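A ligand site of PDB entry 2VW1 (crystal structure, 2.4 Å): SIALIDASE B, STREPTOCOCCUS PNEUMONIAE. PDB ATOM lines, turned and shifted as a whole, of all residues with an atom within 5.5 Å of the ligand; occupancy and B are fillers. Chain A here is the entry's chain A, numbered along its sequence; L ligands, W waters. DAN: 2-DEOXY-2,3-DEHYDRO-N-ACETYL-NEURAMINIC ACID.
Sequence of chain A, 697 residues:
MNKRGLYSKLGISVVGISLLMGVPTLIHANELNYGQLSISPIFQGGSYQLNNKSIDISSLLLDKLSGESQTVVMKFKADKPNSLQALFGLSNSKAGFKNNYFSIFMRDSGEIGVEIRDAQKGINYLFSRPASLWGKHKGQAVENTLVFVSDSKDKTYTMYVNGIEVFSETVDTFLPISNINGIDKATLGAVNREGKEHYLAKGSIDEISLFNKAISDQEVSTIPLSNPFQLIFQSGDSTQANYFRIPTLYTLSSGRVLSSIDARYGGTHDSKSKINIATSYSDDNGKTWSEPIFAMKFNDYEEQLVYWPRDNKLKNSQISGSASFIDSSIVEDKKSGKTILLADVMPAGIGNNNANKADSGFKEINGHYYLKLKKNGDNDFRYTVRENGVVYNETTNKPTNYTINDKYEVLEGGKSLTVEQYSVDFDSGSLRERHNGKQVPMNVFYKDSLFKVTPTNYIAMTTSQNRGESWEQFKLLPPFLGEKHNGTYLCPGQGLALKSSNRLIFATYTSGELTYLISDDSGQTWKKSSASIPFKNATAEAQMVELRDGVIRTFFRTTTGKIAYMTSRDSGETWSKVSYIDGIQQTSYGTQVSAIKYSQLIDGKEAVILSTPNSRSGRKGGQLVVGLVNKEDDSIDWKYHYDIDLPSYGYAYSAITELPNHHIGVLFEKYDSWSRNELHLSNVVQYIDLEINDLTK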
ATOM      1  N   ARG A 245      25.641 -31.089  19.674  1.00  0.00           N
ATOM      2  CA  ARG A 245      24.462 -30.286  19.938  1.00  0.00           C
ATOM      3  C   ARG A 245      24.882 -28.842  20.090  1.00  0.00           C
ATOM      4  O   ARG A 245      26.041 -28.555  20.318  1.00  0.00           O
ATOM      5  CB  ARG A 245      23.757 -30.737  21.231  1.00  0.00           C
ATOM      6  CG  ARG A 245      22.781 -31.918  21.084  1.00  0.00           C
ATOM      7  CD  ARG A 245      21.591 -31.806  22.023  1.00  0.00           C
ATOM      8  NE  ARG A 245      20.773 -30.622  21.704  1.00  0.00           N
ATOM      9  CZ  ARG A 245      19.937 -30.029  22.553  1.00  0.00           C
ATOM     10  NH1 ARG A 245      19.782 -30.506  23.787  1.00  0.00           N
ATOM     11  NH2 ARG A 245      19.255 -28.942  22.179  1.00  0.00           N
ATOM     12  N   ILE A 246      23.900 -27.948  19.975  1.00  0.00           N
ATOM     13  CA  ILE A 246      24.062 -26.541  20.319  1.00  0.00           C
ATOM     14  C   ILE A 246      25.025 -25.858  19.366  1.00  0.00           C
ATOM     15  O   ILE A 246      26.143 -25.465  19.767  1.00  0.00           O
ATOM     16  CB  ILE A 246      24.512 -26.291  21.819  1.00  0.00           C
ATOM     17  CG1 ILE A 246      23.932 -27.321  22.810  1.00  0.00           C
ATOM     18  CG2 ILE A 246      24.175 -24.881  22.249  1.00  0.00           C
ATOM     19  CD1 ILE A 246      22.429 -27.516  22.758  1.00  0.00           C
ATOM     20  N   ASP A 262      28.850 -28.087  20.912  1.00  0.00           N
ATOM     21  CA  ASP A 262      29.086 -29.130  21.898  1.00  0.00           C
ATOM     22  C   ASP A 262      29.506 -30.377  21.170  1.00  0.00           C
ATOM     23  O   ASP A 262      28.720 -30.906  20.383  1.00  0.00           O
ATOM     24  CB  ASP A 262      27.798 -29.508  22.651  1.00  0.00           C
ATOM     25  CG  ASP A 262      27.421 -28.546  23.729  1.00  0.00           C
ATOM     26  OD1 ASP A 262      27.756 -27.339  23.676  1.00  0.00           O
ATOM     27  OD2 ASP A 262      26.721 -28.999  24.639  1.00  0.00           O
ATOM     28  N   ARG A 264      29.624 -33.824  21.998  1.00  0.00           N
ATOM     29  CA  ARG A 264      28.975 -34.582  23.068  1.00  0.00           C
ATOM     30  C   ARG A 264      29.242 -36.043  22.943  1.00  0.00           C
ATOM     31  O   ARG A 264      28.850 -36.661  21.941  1.00  0.00           O
ATOM     32  CB  ARG A 264      27.466 -34.305  23.136  1.00  0.00           C
ATOM     33  CG  ARG A 264      27.151 -32.890  23.560  1.00  0.00           C
ATOM     34  CD  ARG A 264      25.704 -32.693  23.883  1.00  0.00           C
ATOM     35  NE  ARG A 264      25.440 -31.325  24.337  1.00  0.00           N
ATOM     36  CZ  ARG A 264      24.327 -30.946  24.955  1.00  0.00           C
ATOM     37  NH1 ARG A 264      23.353 -31.801  25.210  1.00  0.00           N
ATOM     38  NH2 ARG A 264      24.178 -29.682  25.325  1.00  0.00           N
ATOM     39  N   ASP A 270      22.651 -33.683  28.067  1.00  0.00           N
ATOM     40  CA  ASP A 270      23.239 -32.506  28.676  1.00  0.00           C
ATOM     41  C   ASP A 270      24.235 -33.032  29.672  1.00  0.00           C
ATOM     42  O   ASP A 270      24.193 -34.202  30.028  1.00  0.00           O
ATOM     43  CB  ASP A 270      22.199 -31.696  29.479  1.00  0.00           C
ATOM     44  CG  ASP A 270      21.133 -31.036  28.623  1.00  0.00           C
ATOM     45  OD1 ASP A 270      20.226 -30.441  29.256  1.00  0.00           O
ATOM     46  OD2 ASP A 270      21.173 -31.074  27.369  1.00  0.00           O
ATOM     47  N   SER A 271      25.115 -32.156  30.142  1.00  0.00           N
ATOM     48  CA  SER A 271      25.879 -32.365  31.359  1.00  0.00           C
ATOM     49  C   SER A 271      24.905 -32.732  32.505  1.00  0.00           C
ATOM     50  O   SER A 271      23.838 -32.160  32.582  1.00  0.00           O
ATOM     51  CB  SER A 271      26.623 -31.069  31.677  1.00  0.00           C
ATOM     52  OG  SER A 271      27.693 -30.872  30.784  1.00  0.00           O
ATOM     53  N   ILE A 326      29.557 -26.995  28.189  1.00  0.00           N
ATOM     54  CA  ILE A 326      28.238 -27.045  27.578  1.00  0.00           C
ATOM     55  C   ILE A 326      27.810 -25.615  27.224  1.00  0.00           C
ATOM     56  O   ILE A 326      28.111 -24.674  27.946  1.00  0.00           O
ATOM     57  CB  ILE A 326      27.204 -27.813  28.507  1.00  0.00           C
ATOM     58  CG1 ILE A 326      25.821 -27.952  27.862  1.00  0.00           C
ATOM     59  CG2 ILE A 326      27.131 -27.219  29.936  1.00  0.00           C
ATOM     60  CD1 ILE A 326      25.049 -29.189  28.355  1.00  0.00           C
ATOM     61  N   ASP A 327      27.161 -25.467  26.070  1.00  0.00           N
ATOM     62  CA  ASP A 327      26.598 -24.195  25.589  1.00  0.00           C
ATOM     63  C   ASP A 327      27.658 -23.137  25.333  1.00  0.00           C
ATOM     64  O   ASP A 327      27.978 -22.350  26.228  1.00  0.00           O
ATOM     65  CB  ASP A 327      25.540 -23.615  26.554  1.00  0.00           C
ATOM     66  CG  ASP A 327      24.360 -24.552  26.781  1.00  0.00           C
ATOM     67  OD1 ASP A 327      24.117 -25.473  25.972  1.00  0.00           O
ATOM     68  OD2 ASP A 327      23.679 -24.361  27.817  1.00  0.00           O
ATOM     69  N   ASP A 344      29.657 -22.701  29.403  1.00  0.00           N
ATOM     70  CA  ASP A 344      29.537 -23.224  30.764  1.00  0.00           C
ATOM     71  C   ASP A 344      30.585 -24.323  31.008  1.00  0.00           C
ATOM     72  O   ASP A 344      30.916 -25.086  30.122  1.00  0.00           O
ATOM     73  CB  ASP A 344      28.133 -23.797  31.051  1.00  0.00           C
ATOM     74  CG  ASP A 344      26.979 -22.804  30.797  1.00  0.00           C
ATOM     75  OD1 ASP A 344      27.156 -21.558  30.734  1.00  0.00           O
ATOM     76  OD2 ASP A 344      25.854 -23.325  30.641  1.00  0.00           O
ATOM     77  N   MET A 346      31.476 -27.426  33.727  1.00  0.00           N
ATOM     78  CA  MET A 346      30.876 -28.269  34.750  1.00  0.00           C
ATOM     79  C   MET A 346      31.945 -29.198  35.348  1.00  0.00           C
ATOM     80  O   MET A 346      32.651 -29.907  34.604  1.00  0.00           O
ATOM     81  CB  MET A 346      29.711 -29.081  34.187  1.00  0.00           C
ATOM     82  CG  MET A 346      28.614 -28.255  33.523  1.00  0.00           C
ATOM     83  SD  MET A 346      27.611 -27.434  34.761  1.00  0.00           S
ATOM     84  CE  MET A 346      26.221 -26.853  33.774  1.00  0.00           C
ATOM     85  N   ASN A 352      23.295 -28.952  35.144  1.00  0.00           N
ATOM     86  CA  ASN A 352      22.425 -27.941  35.758  1.00  0.00           C
ATOM     87  C   ASN A 352      21.440 -28.527  36.781  1.00  0.00           C
ATOM     88  O   ASN A 352      20.998 -27.816  37.703  1.00  0.00           O
ATOM     89  CB  ASN A 352      21.699 -27.079  34.714  1.00  0.00           C
ATOM     90  CG  ASN A 352      20.630 -27.846  33.941  1.00  0.00           C
ATOM     91  OD1 ASN A 352      20.632 -29.081  33.887  1.00  0.00           O
ATOM     92  ND2 ASN A 352      19.700 -27.100  33.320  1.00  0.00           N
ATOM     93  N   TYR A 489      23.726 -19.050  33.431  1.00  0.00           N
ATOM     94  CA  TYR A 489      23.929 -19.943  32.328  1.00  0.00           C
ATOM     95  C   TYR A 489      24.008 -19.133  31.022  1.00  0.00           C
ATOM     96  O   TYR A 489      23.117 -18.348  30.706  1.00  0.00           O
ATOM     97  CB  TYR A 489      22.814 -20.984  32.260  1.00  0.00           C
ATOM     98  CG  TYR A 489      22.826 -21.932  33.415  1.00  0.00           C
ATOM     99  CD1 TYR A 489      23.736 -22.995  33.452  1.00  0.00           C
ATOM    100  CD2 TYR A 489      21.942 -21.795  34.495  1.00  0.00           C
ATOM    101  CE1 TYR A 489      23.769 -23.883  34.502  1.00  0.00           C
ATOM    102  CE2 TYR A 489      21.953 -22.694  35.563  1.00  0.00           C
ATOM    103  CZ  TYR A 489      22.878 -23.735  35.564  1.00  0.00           C
ATOM    104  OH  TYR A 489      22.955 -24.639  36.589  1.00  0.00           O
ATOM    105  N   TYR A 509      21.436 -16.395  31.288  1.00  0.00           N
ATOM    106  CA  TYR A 509      20.212 -16.462  32.069  1.00  0.00           C
ATOM    107  C   TYR A 509      20.414 -17.139  33.423  1.00  0.00           C
ATOM    108  O   TYR A 509      21.260 -18.040  33.593  1.00  0.00           O
ATOM    109  CB  TYR A 509      19.097 -17.174  31.294  1.00  0.00           C
ATOM    110  CG  TYR A 509      19.327 -18.652  31.030  1.00  0.00           C
ATOM    111  CD1 TYR A 509      18.908 -19.618  31.950  1.00  0.00           C
ATOM    112  CD2 TYR A 509      19.949 -19.077  29.871  1.00  0.00           C
ATOM    113  CE1 TYR A 509      19.100 -20.963  31.711  1.00  0.00           C
ATOM    114  CE2 TYR A 509      20.156 -20.430  29.628  1.00  0.00           C
ATOM    115  CZ  TYR A 509      19.727 -21.367  30.556  1.00  0.00           C
ATOM    116  OH  TYR A 509      19.912 -22.694  30.303  1.00  0.00           O
ATOM    117  N   THR A 539      14.185 -21.182  31.068  1.00  0.00           N
ATOM    118  CA  THR A 539      15.411 -21.381  30.331  1.00  0.00           C
ATOM    119  C   THR A 539      15.419 -20.259  29.299  1.00  0.00           C
ATOM    120  O   THR A 539      15.150 -20.493  28.123  1.00  0.00           O
ATOM    121  CB  THR A 539      15.413 -22.758  29.630  1.00  0.00           C
ATOM    122  OG1 THR A 539      15.011 -23.778  30.568  1.00  0.00           O
ATOM    123  CG2 THR A 539      16.797 -23.071  29.056  1.00  0.00           C
ATOM    124  N   GLU A 541      16.914 -18.573  27.131  1.00  0.00           N
ATOM    125  CA  GLU A 541      17.990 -18.545  26.150  1.00  0.00           C
ATOM    126  C   GLU A 541      17.780 -17.361  25.203  1.00  0.00           C
ATOM    127  O   GLU A 541      16.784 -17.303  24.487  1.00  0.00           O
ATOM    128  CB  GLU A 541      18.098 -19.882  25.414  1.00  0.00           C
ATOM    129  CG  GLU A 541      18.760 -20.984  26.242  1.00  0.00           C
ATOM    130  CD  GLU A 541      18.453 -22.378  25.752  1.00  0.00           C
ATOM    131  OE1 GLU A 541      19.175 -23.332  26.161  1.00  0.00           O
ATOM    132  OE2 GLU A 541      17.501 -22.540  24.962  1.00  0.00           O
ATOM    133  N   ARG A 557      13.629 -17.354  24.616  1.00  0.00           N
ATOM    134  CA  ARG A 557      12.768 -18.479  24.979  1.00  0.00           C
ATOM    135  C   ARG A 557      12.113 -18.290  26.347  1.00  0.00           C
ATOM    136  O   ARG A 557      12.711 -17.772  27.291  1.00  0.00           O
ATOM    137  CB  ARG A 557      13.642 -19.732  24.999  1.00  0.00           C
ATOM    138  CG  ARG A 557      13.110 -20.946  25.691  1.00  0.00           C
ATOM    139  CD  ARG A 557      14.155 -22.034  25.567  1.00  0.00           C
ATOM    140  NE  ARG A 557      13.748 -23.276  26.202  1.00  0.00           N
ATOM    141  CZ  ARG A 557      14.502 -24.361  26.277  1.00  0.00           C
ATOM    142  NH1 ARG A 557      15.716 -24.371  25.753  1.00  0.00           N
ATOM    143  NH2 ARG A 557      14.043 -25.437  26.876  1.00  0.00           N
ATOM    144  N   GLY A 590       9.831 -24.807  25.317  1.00  0.00           N
ATOM    145  CA  GLY A 590      10.568 -23.936  24.407  1.00  0.00           C
ATOM    146  C   GLY A 590      11.854 -24.486  23.830  1.00  0.00           C
ATOM    147  O   GLY A 590      12.304 -25.587  24.174  1.00  0.00           O
ATOM    148  N   ARG A 619       9.784 -29.833  18.850  1.00  0.00           N
ATOM    149  CA  ARG A 619      10.839 -29.069  18.194  1.00  0.00           C
ATOM    150  C   ARG A 619      10.919 -29.539  16.753  1.00  0.00           C
ATOM    151  O   ARG A 619      11.702 -30.420  16.407  1.00  0.00           O
ATOM    152  CB  ARG A 619      12.176 -29.241  18.916  1.00  0.00           C
ATOM    153  CG  ARG A 619      12.132 -28.890  20.371  1.00  0.00           C
ATOM    154  CD  ARG A 619      13.495 -28.879  20.977  1.00  0.00           C
ATOM    155  NE  ARG A 619      13.468 -28.149  22.231  1.00  0.00           N
ATOM    156  CZ  ARG A 619      14.450 -28.185  23.130  1.00  0.00           C
ATOM    157  NH1 ARG A 619      15.518 -28.935  22.920  1.00  0.00           N
ATOM    158  NH2 ARG A 619      14.323 -27.495  24.257  1.00  0.00           N
ATOM    159  N   TYR A 653      17.753 -26.454  18.217  1.00  0.00           N
ATOM    160  CA  TYR A 653      18.683 -25.335  18.386  1.00  0.00           C
ATOM    161  C   TYR A 653      19.287 -24.957  17.045  1.00  0.00           C
ATOM    162  O   TYR A 653      19.467 -25.811  16.175  1.00  0.00           O
ATOM    163  CB  TYR A 653      19.779 -25.656  19.399  1.00  0.00           C
ATOM    164  CG  TYR A 653      19.367 -25.541  20.854  1.00  0.00           C
ATOM    165  CD1 TYR A 653      18.082 -25.925  21.270  1.00  0.00           C
ATOM    166  CD2 TYR A 653      20.259 -25.088  21.833  1.00  0.00           C
ATOM    167  CE1 TYR A 653      17.698 -25.837  22.572  1.00  0.00           C
ATOM    168  CE2 TYR A 653      19.889 -25.013  23.159  1.00  0.00           C
ATOM    169  CZ  TYR A 653      18.605 -25.378  23.521  1.00  0.00           C
ATOM    170  OH  TYR A 653      18.200 -25.311  24.836  1.00  0.00           O
ATOM    171  N   SER A 673      15.332 -32.445  19.788  1.00  0.00           N
ATOM    172  CA  SER A 673      16.358 -32.672  20.830  1.00  0.00           C
ATOM    173  C   SER A 673      15.817 -32.623  22.240  1.00  0.00           C
ATOM    174  O   SER A 673      16.580 -32.584  23.199  1.00  0.00           O
ATOM    175  CB  SER A 673      17.548 -31.711  20.682  1.00  0.00           C
ATOM    176  OG  SER A 673      17.161 -30.357  20.796  1.00  0.00           O
ATOM    177  N   TRP A 674      14.480 -32.604  22.341  1.00  0.00           N
ATOM    178  CA  TRP A 674      13.759 -32.675  23.611  1.00  0.00           C
ATOM    179  C   TRP A 674      13.176 -34.058  23.778  1.00  0.00           C
ATOM    180  O   TRP A 674      13.128 -34.598  24.895  1.00  0.00           O
ATOM    181  CB  TRP A 674      12.614 -31.632  23.637  1.00  0.00           C
ATOM    182  CG  TRP A 674      11.933 -31.479  24.985  1.00  0.00           C
ATOM    183  CD1 TRP A 674      10.724 -32.038  25.376  1.00  0.00           C
ATOM    184  CD2 TRP A 674      12.412 -30.727  26.110  1.00  0.00           C
ATOM    185  NE1 TRP A 674      10.435 -31.665  26.674  1.00  0.00           N
ATOM    186  CE2 TRP A 674      11.447 -30.862  27.152  1.00  0.00           C
ATOM    187  CE3 TRP A 674      13.553 -29.954  26.351  1.00  0.00           C
ATOM    188  CZ2 TRP A 674      11.604 -30.239  28.418  1.00  0.00           C
ATOM    189  CZ3 TRP A 674      13.711 -29.340  27.612  1.00  0.00           C
ATOM    190  CH2 TRP A 674      12.741 -29.491  28.620  1.00  0.00           C
HETATM  191  C1  DAN L   1      17.605 -28.217  25.582  1.00  0.00           C
HETATM  192  C2  DAN L   1      18.752 -27.810  26.412  1.00  0.00           C
HETATM  193  C3  DAN L   1      20.012 -27.670  25.956  1.00  0.00           C
HETATM  194  C4  DAN L   1      21.166 -27.175  26.835  1.00  0.00           C
HETATM  195  C5  DAN L   1      20.875 -27.307  28.337  1.00  0.00           C
HETATM  196  C6  DAN L   1      19.439 -26.792  28.546  1.00  0.00           C
HETATM  197  C7  DAN L   1      19.031 -26.854  30.006  1.00  0.00           C
HETATM  198  C8  DAN L   1      17.653 -26.302  30.341  1.00  0.00           C
HETATM  199  C9  DAN L   1      16.483 -27.182  29.878  1.00  0.00           C
HETATM  200  C10 DAN L   1      22.476 -26.846  30.241  1.00  0.00           C
HETATM  201  C11 DAN L   1      23.414 -25.824  30.809  1.00  0.00           C
HETATM  202  N5  DAN L   1      21.797 -26.472  29.133  1.00  0.00           N
HETATM  203  O1A DAN L   1      17.676 -28.965  24.569  1.00  0.00           O
HETATM  204  O1B DAN L   1      16.496 -27.762  25.902  1.00  0.00           O
HETATM  205  O4  DAN L   1      22.471 -27.630  26.360  1.00  0.00           O
HETATM  206  O6  DAN L   1      18.467 -27.541  27.815  1.00  0.00           O
HETATM  207  O7  DAN L   1      19.167 -28.199  30.474  1.00  0.00           O
HETATM  208  O8  DAN L   1      17.619 -26.212  31.771  1.00  0.00           O
HETATM  209  O9  DAN L   1      15.958 -26.805  28.601  1.00  0.00           O
HETATM  210  O10 DAN L   1      22.409 -27.940  30.786  1.00  0.00           O
HETATM  211  O   HOH W   1      20.953 -24.579  32.474  1.00  0.00           O
HETATM  212  O   HOH W   2      23.712 -29.414  32.326  1.00  0.00           O
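CD1 of Ile 246 touches O4 of the ligand, at 3.6 Å.
Ile 326 touches the ligand (CD1 to O4, 3.6 Å).
Asp 344 touches the ligand (OD2 to C11, 3.5 Å).
CD1 of Tyr 489 touches C11 of the ligand, at 3.9 Å.
Thr 539 touches the ligand (CG2 to C8, 3.6 Å).
Trp 674 touches the ligand (CZ3 to O9, 3.5 Å).
Hydrophobic or aromatic side chains that line the ligand: Ile 246, Ile 326, Tyr 489, Tyr 653 and Trp 674.
Of the 21 residues printed, 14 come within 4 Å of the ligand.
The nearest printed residue that does not touch the ligand is Ser 673 (4.02 Å).
The side-chain carboxylate (OD1) of Asp 270 sits at hydrogen-bond distance from an oxygen (O7) of the ligand, at 2.8 Å.
O1B of the ligand lies close to OH of Tyr 653, at 3.2 Å.
The side-chain amide nitrogen of Asn 352 sits at hydrogen-bond distance from an oxygen (O8) of the ligand.
NH1 of Arg 557 is in salt-bridge range of O1B of the ligand (3.5 Å).
O1A of the ligand lies within salt-bridge range of NH1 of Arg 245 (2.7 Å).
The side-chain carboxylate (OD1) of Asp 327 sits at hydrogen-bond distance from an oxygen (O4) of the ligand.
An oxygen (O1A) of the ligand lies within salt-bridge range of the guanidinium group of Arg 619 (2.7 Å).
The guanidinium group of Arg 264 lies within hydrogen-bond range of an oxygen (O4) of the ligand.
NE of Arg 264 lies within salt-bridge range of OD2 of Asp 262 (2.7 Å).
OH of Tyr 653 sits at hydrogen-bond distance from OE1 of Glu 541 (2.6 Å).
NH1 of Arg 619 is in hydrogen-bond range of OG of Ser 673.
The guanidinium group (NH1) of Arg 245 lies within salt-bridge range of the side-chain carboxylate (OD2) of Asp 270, at 3.9 Å.
NH2 of Arg 557 sits at hydrogen-bond distance from O of Gly 590.
The backbone carbonyl oxygen (O) of Gly 590 is in hydrogen-bond range of the guanidinium group (NH2) of Arg 619, 2.8 Å away.
The backbone carbonyl oxygen (O) of Arg 245 sits at hydrogen-bond distance from the backbone NH (N) of Asp 262, at 2.9 Å.
N of Asp 344 sits at hydrogen-bond distance from O of Ile 326, at 2.9 Å.
Water W2 lies within hydrogen-bond range of an oxygen (O10) of the ligand (2.5 Å), the backbone carbonyl oxygen (O) of Ser 271 (2.8 Å) and the backbone NH (N) of Asn 352 (2.9 Å).
Water W1 bridges ND2 of Asn 352 (2.9 Å) and OH of Tyr 509 (3.1 Å).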
